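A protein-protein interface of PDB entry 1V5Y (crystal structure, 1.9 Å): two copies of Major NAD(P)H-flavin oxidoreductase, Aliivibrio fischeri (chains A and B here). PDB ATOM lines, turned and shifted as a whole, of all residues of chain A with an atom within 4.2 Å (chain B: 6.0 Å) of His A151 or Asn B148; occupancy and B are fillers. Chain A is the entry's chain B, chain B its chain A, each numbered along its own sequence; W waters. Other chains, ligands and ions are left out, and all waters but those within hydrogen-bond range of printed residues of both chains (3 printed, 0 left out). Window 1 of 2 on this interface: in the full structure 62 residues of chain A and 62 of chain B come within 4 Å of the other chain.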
ATOM      1  N   LEU A   8     -13.261  11.860  -8.852  1.00  0.00           N
ATOM      2  CA  LEU A   8     -13.296  12.164 -10.284  1.00  0.00           C
ATOM      3  C   LEU A   8     -14.667  12.059 -10.920  1.00  0.00           C
ATOM      4  O   LEU A   8     -14.910  12.660 -11.961  1.00  0.00           O
ATOM      5  CB  LEU A   8     -12.257  11.350 -11.045  1.00  0.00           C
ATOM      6  CG  LEU A   8     -10.830  11.636 -10.566  1.00  0.00           C
ATOM      7  CD1 LEU A   8      -9.875  10.732 -11.307  1.00  0.00           C
ATOM      8  CD2 LEU A   8     -10.455  13.106 -10.770  1.00  0.00           C
ATOM      9  N   GLY A 147      -4.168  19.833 -14.859  1.00  0.00           N
ATOM     10  CA  GLY A 147      -4.759  18.530 -14.567  1.00  0.00           C
ATOM     11  C   GLY A 147      -4.536  18.197 -13.100  1.00  0.00           C
ATOM     12  O   GLY A 147      -5.390  17.626 -12.438  1.00  0.00           O
ATOM     13  N   ASN A 148      -3.360  18.559 -12.603  1.00  0.00           N
ATOM     14  CA  ASN A 148      -3.012  18.370 -11.214  1.00  0.00           C
ATOM     15  C   ASN A 148      -3.964  19.230 -10.365  1.00  0.00           C
ATOM     16  O   ASN A 148      -4.550  18.755  -9.400  1.00  0.00           O
ATOM     17  CB  ASN A 148      -1.560  18.790 -11.005  1.00  0.00           C
ATOM     18  CG  ASN A 148      -1.088  18.558  -9.604  1.00  0.00           C
ATOM     19  OD1 ASN A 148      -1.462  17.578  -8.974  1.00  0.00           O
ATOM     20  ND2 ASN A 148      -0.251  19.451  -9.104  1.00  0.00           N
ATOM     21  N   ALA A 149      -4.186  20.474 -10.782  1.00  0.00           N
ATOM     22  CA  ALA A 149      -5.075  21.374 -10.053  1.00  0.00           C
ATOM     23  C   ALA A 149      -6.514  20.880  -9.984  1.00  0.00           C
ATOM     24  O   ALA A 149      -7.158  20.989  -8.942  1.00  0.00           O
ATOM     25  CB  ALA A 149      -5.036  22.776 -10.673  1.00  0.00           C
ATOM     26  N   LEU A 150      -7.023  20.337 -11.084  1.00  0.00           N
ATOM     27  CA  LEU A 150      -8.401  19.861 -11.104  1.00  0.00           C
ATOM     28  C   LEU A 150      -8.614  18.674 -10.162  1.00  0.00           C
ATOM     29  O   LEU A 150      -9.658  18.566  -9.513  1.00  0.00           O
ATOM     30  CB  LEU A 150      -8.834  19.521 -12.536  1.00  0.00           C
ATOM     31  CG  LEU A 150      -9.045  20.693 -13.499  1.00  0.00           C
ATOM     32  CD1 LEU A 150      -9.354  20.137 -14.877  1.00  0.00           C
ATOM     33  CD2 LEU A 150     -10.161  21.610 -13.032  1.00  0.00           C
ATOM     34  N   HIS A 151      -7.606  17.818 -10.058  1.00  0.00           N
ATOM     35  CA  HIS A 151      -7.678  16.666  -9.173  1.00  0.00           C
ATOM     36  C   HIS A 151      -7.582  17.200  -7.733  1.00  0.00           C
ATOM     37  O   HIS A 151      -8.306  16.747  -6.863  1.00  0.00           O
ATOM     38  CB  HIS A 151      -6.526  15.692  -9.478  1.00  0.00           C
ATOM     39  CG  HIS A 151      -6.705  14.329  -8.864  1.00  0.00           C
ATOM     40  ND1 HIS A 151      -6.548  13.158  -9.579  1.00  0.00           N
ATOM     41  CD2 HIS A 151      -7.023  13.952  -7.600  1.00  0.00           C
ATOM     42  CE1 HIS A 151      -6.754  12.122  -8.786  1.00  0.00           C
ATOM     43  NE2 HIS A 151      -7.044  12.577  -7.579  1.00  0.00           N
ATOM     44  N   THR A 152      -6.699  18.178  -7.504  1.00  0.00           N
ATOM     45  CA  THR A 152      -6.517  18.799  -6.188  1.00  0.00           C
ATOM     46  C   THR A 152      -7.815  19.437  -5.676  1.00  0.00           C
ATOM     47  O   THR A 152      -8.179  19.248  -4.511  1.00  0.00           O
ATOM     48  CB  THR A 152      -5.417  19.856  -6.221  1.00  0.00           C
ATOM     49  OG1 THR A 152      -4.158  19.217  -6.454  1.00  0.00           O
ATOM     50  CG2 THR A 152      -5.358  20.622  -4.890  1.00  0.00           C
ATOM     51  N   LEU A 153      -8.517  20.162  -6.548  1.00  0.00           N
ATOM     52  CA  LEU A 153      -9.791  20.811  -6.202  1.00  0.00           C
ATOM     53  C   LEU A 153     -10.885  19.795  -5.897  1.00  0.00           C
ATOM     54  O   LEU A 153     -11.767  20.046  -5.062  1.00  0.00           O
ATOM     55  CB  LEU A 153     -10.239  21.742  -7.324  1.00  0.00           C
ATOM     56  CG  LEU A 153      -9.391  23.009  -7.506  1.00  0.00           C
ATOM     57  CD1 LEU A 153      -9.656  23.634  -8.874  1.00  0.00           C
ATOM     58  CD2 LEU A 153      -9.696  23.999  -6.387  1.00  0.00           C
ATOM     59  N   ALA A 154     -10.841  18.648  -6.579  1.00  0.00           N
ATOM     60  CA  ALA A 154     -11.817  17.581  -6.346  1.00  0.00           C
ATOM     61  C   ALA A 154     -11.618  17.057  -4.921  1.00  0.00           C
ATOM     62  O   ALA A 154     -12.578  16.803  -4.209  1.00  0.00           O
ATOM     63  CB  ALA A 154     -11.624  16.447  -7.363  1.00  0.00           C
ATOM     64  N   ARG A 155     -10.370  16.940  -4.489  1.00  0.00           N
ATOM     65  CA  ARG A 155     -10.076  16.467  -3.136  1.00  0.00           C
ATOM     66  C   ARG A 155     -10.460  17.475  -2.040  1.00  0.00           C
ATOM     67  O   ARG A 155     -10.790  17.070  -0.930  1.00  0.00           O
ATOM     68  CB  ARG A 155      -8.594  16.103  -3.010  1.00  0.00           C
ATOM     69  CG  ARG A 155      -8.192  14.976  -3.934  1.00  0.00           C
ATOM     70  CD  ARG A 155      -6.750  14.625  -3.771  1.00  0.00           C
ATOM     71  NE  ARG A 155      -6.479  13.952  -2.509  1.00  0.00           N
ATOM     72  CZ  ARG A 155      -5.279  13.516  -2.156  1.00  0.00           C
ATOM     73  NH1 ARG A 155      -4.250  13.682  -2.977  1.00  0.00           N
ATOM     74  NH2 ARG A 155      -5.090  12.937  -0.980  1.00  0.00           N
ATOM     75  N   ALA B  34      -9.599   6.538 -14.104  1.00  0.00           N
ATOM     76  CA  ALA B  34      -9.236   7.918 -13.746  1.00  0.00           C
ATOM     77  C   ALA B  34      -8.830   8.703 -15.013  1.00  0.00           C
ATOM     78  O   ALA B  34      -9.187   9.868 -15.182  1.00  0.00           O
ATOM     79  CB  ALA B  34      -8.108   7.912 -12.735  1.00  0.00           C
ATOM     80  N   LEU B  35      -8.113   8.045 -15.921  1.00  0.00           N
ATOM     81  CA  LEU B  35      -7.698   8.651 -17.182  1.00  0.00           C
ATOM     82  C   LEU B  35      -8.914   8.955 -18.035  1.00  0.00           C
ATOM     83  O   LEU B  35      -9.002  10.029 -18.632  1.00  0.00           O
ATOM     84  CB  LEU B  35      -6.762   7.720 -17.962  1.00  0.00           C
ATOM     85  CG  LEU B  35      -5.303   7.601 -17.506  1.00  0.00           C
ATOM     86  CD1 LEU B  35      -4.554   6.657 -18.436  1.00  0.00           C
ATOM     87  CD2 LEU B  35      -4.649   8.972 -17.527  1.00  0.00           C
ATOM     88  N   LEU B  37     -11.951   9.587 -17.071  1.00  0.00           N
ATOM     89  CA  LEU B  37     -12.733  10.670 -16.462  1.00  0.00           C
ATOM     90  C   LEU B  37     -12.105  12.060 -16.532  1.00  0.00           C
ATOM     91  O   LEU B  37     -12.711  13.019 -16.080  1.00  0.00           O
ATOM     92  CB  LEU B  37     -13.065  10.346 -15.009  1.00  0.00           C
ATOM     93  CG  LEU B  37     -13.929   9.108 -14.811  1.00  0.00           C
ATOM     94  CD1 LEU B  37     -13.945   8.733 -13.335  1.00  0.00           C
ATOM     95  CD2 LEU B  37     -15.331   9.389 -15.329  1.00  0.00           C
ATOM     96  N   SER B  38     -10.909  12.163 -17.104  1.00  0.00           N
ATOM     97  CA  SER B  38     -10.223  13.448 -17.255  1.00  0.00           C
ATOM     98  C   SER B  38     -11.064  14.440 -18.046  1.00  0.00           C
ATOM     99  O   SER B  38     -11.767  14.076 -19.003  1.00  0.00           O
ATOM    100  CB  SER B  38      -8.888  13.272 -17.969  1.00  0.00           C
ATOM    101  OG  SER B  38      -8.053  12.356 -17.302  1.00  0.00           O
ATOM    102  N   ALA B  39     -10.996  15.701 -17.623  1.00  0.00           N
ATOM    103  CA  ALA B  39     -11.718  16.781 -18.261  1.00  0.00           C
ATOM    104  C   ALA B  39     -10.954  17.211 -19.513  1.00  0.00           C
ATOM    105  O   ALA B  39      -9.738  17.018 -19.609  1.00  0.00           O
ATOM    106  CB  ALA B  39     -11.824  17.953 -17.286  1.00  0.00           C
ATOM    107  N   TYR B 143      -1.911  16.227 -22.029  1.00  0.00           N
ATOM    108  CA  TYR B 143      -1.045  16.576 -20.900  1.00  0.00           C
ATOM    109  C   TYR B 143      -1.869  16.861 -19.639  1.00  0.00           C
ATOM    110  O   TYR B 143      -1.384  16.691 -18.530  1.00  0.00           O
ATOM    111  CB  TYR B 143      -0.137  17.758 -21.234  1.00  0.00           C
ATOM    112  CG  TYR B 143       1.135  17.322 -21.883  1.00  0.00           C
ATOM    113  CD1 TYR B 143       1.123  16.705 -23.146  1.00  0.00           C
ATOM    114  CD2 TYR B 143       2.356  17.506 -21.247  1.00  0.00           C
ATOM    115  CE1 TYR B 143       2.297  16.290 -23.753  1.00  0.00           C
ATOM    116  CE2 TYR B 143       3.529  17.097 -21.835  1.00  0.00           C
ATOM    117  CZ  TYR B 143       3.493  16.491 -23.094  1.00  0.00           C
ATOM    118  OH  TYR B 143       4.669  16.120 -23.676  1.00  0.00           O
ATOM    119  N   LEU B 144      -3.104  17.314 -19.814  1.00  0.00           N
ATOM    120  CA  LEU B 144      -3.983  17.535 -18.680  1.00  0.00           C
ATOM    121  C   LEU B 144      -4.311  16.153 -18.076  1.00  0.00           C
ATOM    122  O   LEU B 144      -4.293  15.972 -16.851  1.00  0.00           O
ATOM    123  CB  LEU B 144      -5.254  18.245 -19.131  1.00  0.00           C
ATOM    124  CG  LEU B 144      -6.208  18.734 -18.034  1.00  0.00           C
ATOM    125  CD1 LEU B 144      -7.177  19.707 -18.662  1.00  0.00           C
ATOM    126  CD2 LEU B 144      -6.974  17.564 -17.361  1.00  0.00           C
ATOM    127  N   ALA B 145      -4.583  15.175 -18.942  1.00  0.00           N
ATOM    128  CA  ALA B 145      -4.878  13.810 -18.506  1.00  0.00           C
ATOM    129  C   ALA B 145      -3.642  13.235 -17.802  1.00  0.00           C
ATOM    130  O   ALA B 145      -3.768  12.515 -16.822  1.00  0.00           O
ATOM    131  CB  ALA B 145      -5.291  12.934 -19.714  1.00  0.00           C
ATOM    132  N   LEU B 146      -2.450  13.590 -18.275  1.00  0.00           N
ATOM    133  CA  LEU B 146      -1.211  13.128 -17.664  1.00  0.00           C
ATOM    134  C   LEU B 146      -1.050  13.718 -16.252  1.00  0.00           C
ATOM    135  O   LEU B 146      -0.607  13.017 -15.326  1.00  0.00           O
ATOM    136  CB  LEU B 146      -0.011  13.486 -18.530  1.00  0.00           C
ATOM    137  CG  LEU B 146       1.402  13.228 -17.993  1.00  0.00           C
ATOM    138  CD1 LEU B 146       1.650  11.733 -17.671  1.00  0.00           C
ATOM    139  CD2 LEU B 146       2.408  13.726 -19.024  1.00  0.00           C
ATOM    140  N   GLY B 147      -1.405  14.995 -16.090  1.00  0.00           N
ATOM    141  CA  GLY B 147      -1.320  15.638 -14.780  1.00  0.00           C
ATOM    142  C   GLY B 147      -2.265  14.952 -13.810  1.00  0.00           C
ATOM    143  O   GLY B 147      -1.969  14.803 -12.628  1.00  0.00           O
ATOM    144  N   ASN B 148      -3.412  14.540 -14.331  1.00  0.00           N
ATOM    145  CA  ASN B 148      -4.420  13.835 -13.561  1.00  0.00           C
ATOM    146  C   ASN B 148      -3.851  12.465 -13.182  1.00  0.00           C
ATOM    147  O   ASN B 148      -3.960  12.031 -12.042  1.00  0.00           O
ATOM    148  CB  ASN B 148      -5.687  13.667 -14.411  1.00  0.00           C
ATOM    149  CG  ASN B 148      -6.842  13.059 -13.641  1.00  0.00           C
ATOM    150  OD1 ASN B 148      -7.024  13.336 -12.459  1.00  0.00           O
ATOM    151  ND2 ASN B 148      -7.650  12.248 -14.318  1.00  0.00           N
ATOM    152  N   ALA B 149      -3.203  11.803 -14.133  1.00  0.00           N
ATOM    153  CA  ALA B 149      -2.637  10.486 -13.884  1.00  0.00           C
ATOM    154  C   ALA B 149      -1.530  10.519 -12.841  1.00  0.00           C
ATOM    155  O   ALA B 149      -1.421   9.614 -12.023  1.00  0.00           O
ATOM    156  CB  ALA B 149      -2.108   9.864 -15.191  1.00  0.00           C
ATOM    157  N   LEU B 150      -0.688  11.546 -12.876  1.00  0.00           N
ATOM    158  CA  LEU B 150       0.403  11.617 -11.916  1.00  0.00           C
ATOM    159  C   LEU B 150      -0.119  11.816 -10.486  1.00  0.00           C
ATOM    160  O   LEU B 150       0.454  11.295  -9.533  1.00  0.00           O
ATOM    161  CB  LEU B 150       1.390  12.718 -12.300  1.00  0.00           C
ATOM    162  CG  LEU B 150       2.274  12.455 -13.524  1.00  0.00           C
ATOM    163  CD1 LEU B 150       3.065  13.726 -13.803  1.00  0.00           C
ATOM    164  CD2 LEU B 150       3.229  11.262 -13.300  1.00  0.00           C
ATOM    165  N   HIS B 151      -1.219  12.546 -10.351  1.00  0.00           N
ATOM    166  CA  HIS B 151      -1.803  12.781  -9.038  1.00  0.00           C
ATOM    167  C   HIS B 151      -2.469  11.461  -8.599  1.00  0.00           C
ATOM    168  O   HIS B 151      -2.364  11.061  -7.456  1.00  0.00           O
ATOM    169  CB  HIS B 151      -2.833  13.931  -9.104  1.00  0.00           C
ATOM    170  CG  HIS B 151      -3.238  14.462  -7.762  1.00  0.00           C
ATOM    171  ND1 HIS B 151      -3.273  15.814  -7.474  1.00  0.00           N
ATOM    172  CD2 HIS B 151      -3.631  13.828  -6.631  1.00  0.00           C
ATOM    173  CE1 HIS B 151      -3.673  15.988  -6.228  1.00  0.00           C
ATOM    174  NE2 HIS B 151      -3.896  14.800  -5.694  1.00  0.00           N
ATOM    175  N   THR B 152      -3.105  10.770  -9.541  1.00  0.00           N
ATOM    176  CA  THR B 152      -3.771   9.509  -9.260  1.00  0.00           C
ATOM    177  C   THR B 152      -2.774   8.466  -8.775  1.00  0.00           C
ATOM    178  O   THR B 152      -3.039   7.746  -7.816  1.00  0.00           O
ATOM    179  CB  THR B 152      -4.499   8.977 -10.499  1.00  0.00           C
ATOM    180  OG1 THR B 152      -5.584   9.849 -10.824  1.00  0.00           O
ATOM    181  CG2 THR B 152      -5.047   7.565 -10.237  1.00  0.00           C
ATOM    182  N   LEU B 153      -1.623   8.391  -9.432  1.00  0.00           N
ATOM    183  CA  LEU B 153      -0.573   7.442  -9.059  1.00  0.00           C
ATOM    184  C   LEU B 153       0.020   7.729  -7.686  1.00  0.00           C
ATOM    185  O   LEU B 153       0.416   6.806  -6.977  1.00  0.00           O
ATOM    186  CB  LEU B 153       0.533   7.428 -10.103  1.00  0.00           C
ATOM    187  CG  LEU B 153       0.161   6.747 -11.441  1.00  0.00           C
ATOM    188  CD1 LEU B 153       1.155   7.144 -12.531  1.00  0.00           C
ATOM    189  CD2 LEU B 153       0.101   5.227 -11.283  1.00  0.00           C
ATOM    190  N   ARG B 155      -1.680   8.951  -5.215  1.00  0.00           N
ATOM    191  CA  ARG B 155      -2.674   8.462  -4.257  1.00  0.00           C
ATOM    192  C   ARG B 155      -2.674   6.946  -4.087  1.00  0.00           C
ATOM    193  O   ARG B 155      -3.015   6.447  -3.024  1.00  0.00           O
ATOM    194  CB  ARG B 155      -4.074   8.940  -4.648  1.00  0.00           C
ATOM    195  CG  ARG B 155      -4.215  10.457  -4.599  1.00  0.00           C
ATOM    196  CD  ARG B 155      -5.589  10.883  -4.979  1.00  0.00           C
ATOM    197  NE  ARG B 155      -6.556  10.559  -3.944  1.00  0.00           N
ATOM    198  CZ  ARG B 155      -7.836  10.888  -4.032  1.00  0.00           C
ATOM    199  NH1 ARG B 155      -8.276  11.536  -5.097  1.00  0.00           N
ATOM    200  NH2 ARG B 155      -8.683  10.578  -3.072  1.00  0.00           N
HETATM  201  O   HOH W   1      -7.728  16.139 -13.239  1.00  0.00           O
HETATM  202  O   HOH W   2     -13.483  14.021 -13.643  1.00  0.00           O
HETATM  203  O   HOH W   3       0.137  15.760 -10.901  1.00  0.00           O
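His A151 touches four residues of chain B. Of the printed residues of chain A, Asn B148 touches Leu A8 (3.8 Å) and His A151 (2.9 Å). Of the printed residues of chain B, Leu A8 touches Ala B34 (3.6 Å), Leu B37 (3.9 Å) and Asn B148 (3.8 Å). Of the printed residues of chain B, Asn A148 touches Gly B147 and His B151.
Of the 17 printed residues of chain B, 8 touch a printed residue of chain A. Printed residues of chain B that touch a printed residue of chain A: Ala B34, Leu B37, Leu B144, Gly B147, Asn B148, His B151, Thr B152 and Arg B155. Hydrophobic or aromatic side chains of chain B that line the printed part of chain A: Ala B34, Leu B37, Leu B144 and His B151. Among the printed residues, 13 pairs touch across the chains. Among the printed residues, no Asp or Glu carboxylate lies within 4 Å of a Lys or Arg side-chain nitrogen of the other chain.
Water W2 lies within hydrogen-bond range of O of Leu A8 and O of Leu B37. Water W1 lies within hydrogen-bond range of the backbone carbonyl oxygen of Gly A147 (2.9 Å) and the side-chain amide oxygen of Asn B148 (3.0 Å). Water W3 bridges O of Gly B147 and OD1 of Asn A148.
The side-chain amide oxygen (OD1) of Asn B148 lies within hydrogen-bond range of a ring nitrogen (ND1) of His A151, 2.9 Å away. ND1 of His B151 is in hydrogen-bond range of OD1 of Asn A148, 2.9 Å away. A ring nitrogen (NE2) of His B151 sits at hydrogen-bond distance from the guanidinium group (NH1) of Arg A155. A ring nitrogen (NE2) of His A151 lies within hydrogen-bond range of the guanidinium group (NH1) of Arg B155, 3.0 Å away.
The side-chain hydroxyl (OG) of Ser B38 is in hydrogen-bond range of the backbone carbonyl oxygen (O) of Ala B34, at 3.5 Å. The side-chain amide nitrogen (ND2) of Asn B148 sits at hydrogen-bond distance from the backbone carbonyl oxygen (O) of Ala B34 (3.0 Å). ND2 of Asn B148 lies within hydrogen-bond range of OG of Ser B38 (3.0 Å). O of Asn B148 is in hydrogen-bond range of OG1 of Thr B152 (3.0 Å). O of Asn A148 sits at hydrogen-bond distance from OG1 of Thr A152.
Asn A148 touches His B151, and with the chains exchanged His A151 touches Asn B148. His A151 touches Thr B152, and with the chains exchanged Thr A152 touches His B151. His A151 touches Arg B155, and with the chains exchanged Arg A155 touches His B151. Arg A155 touches its own counterpart, Arg B155. 8 positions are printed for both chains. Of the 13 pairs that touch across the chains among the printed residues, 8 have their exchanged pair printed and touching as well.
Among the printed residues, merely in contact across the chains: Leu A8 with Ala B34 (3.6 Å), Leu A8 with Leu B37 (3.9 Å), Leu A8 with Asn B148 (3.8 Å), Gly A147 with Leu B144 (3.5 Å), Asn A148 with Gly B147 (3.96 Å), His A151 with His B151 (3.5 Å), His A151 with Thr B152 (3.3 Å), Thr A152 with His B151 (3.3 Å) and Arg A155 with Arg B155 (3.6 Å).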
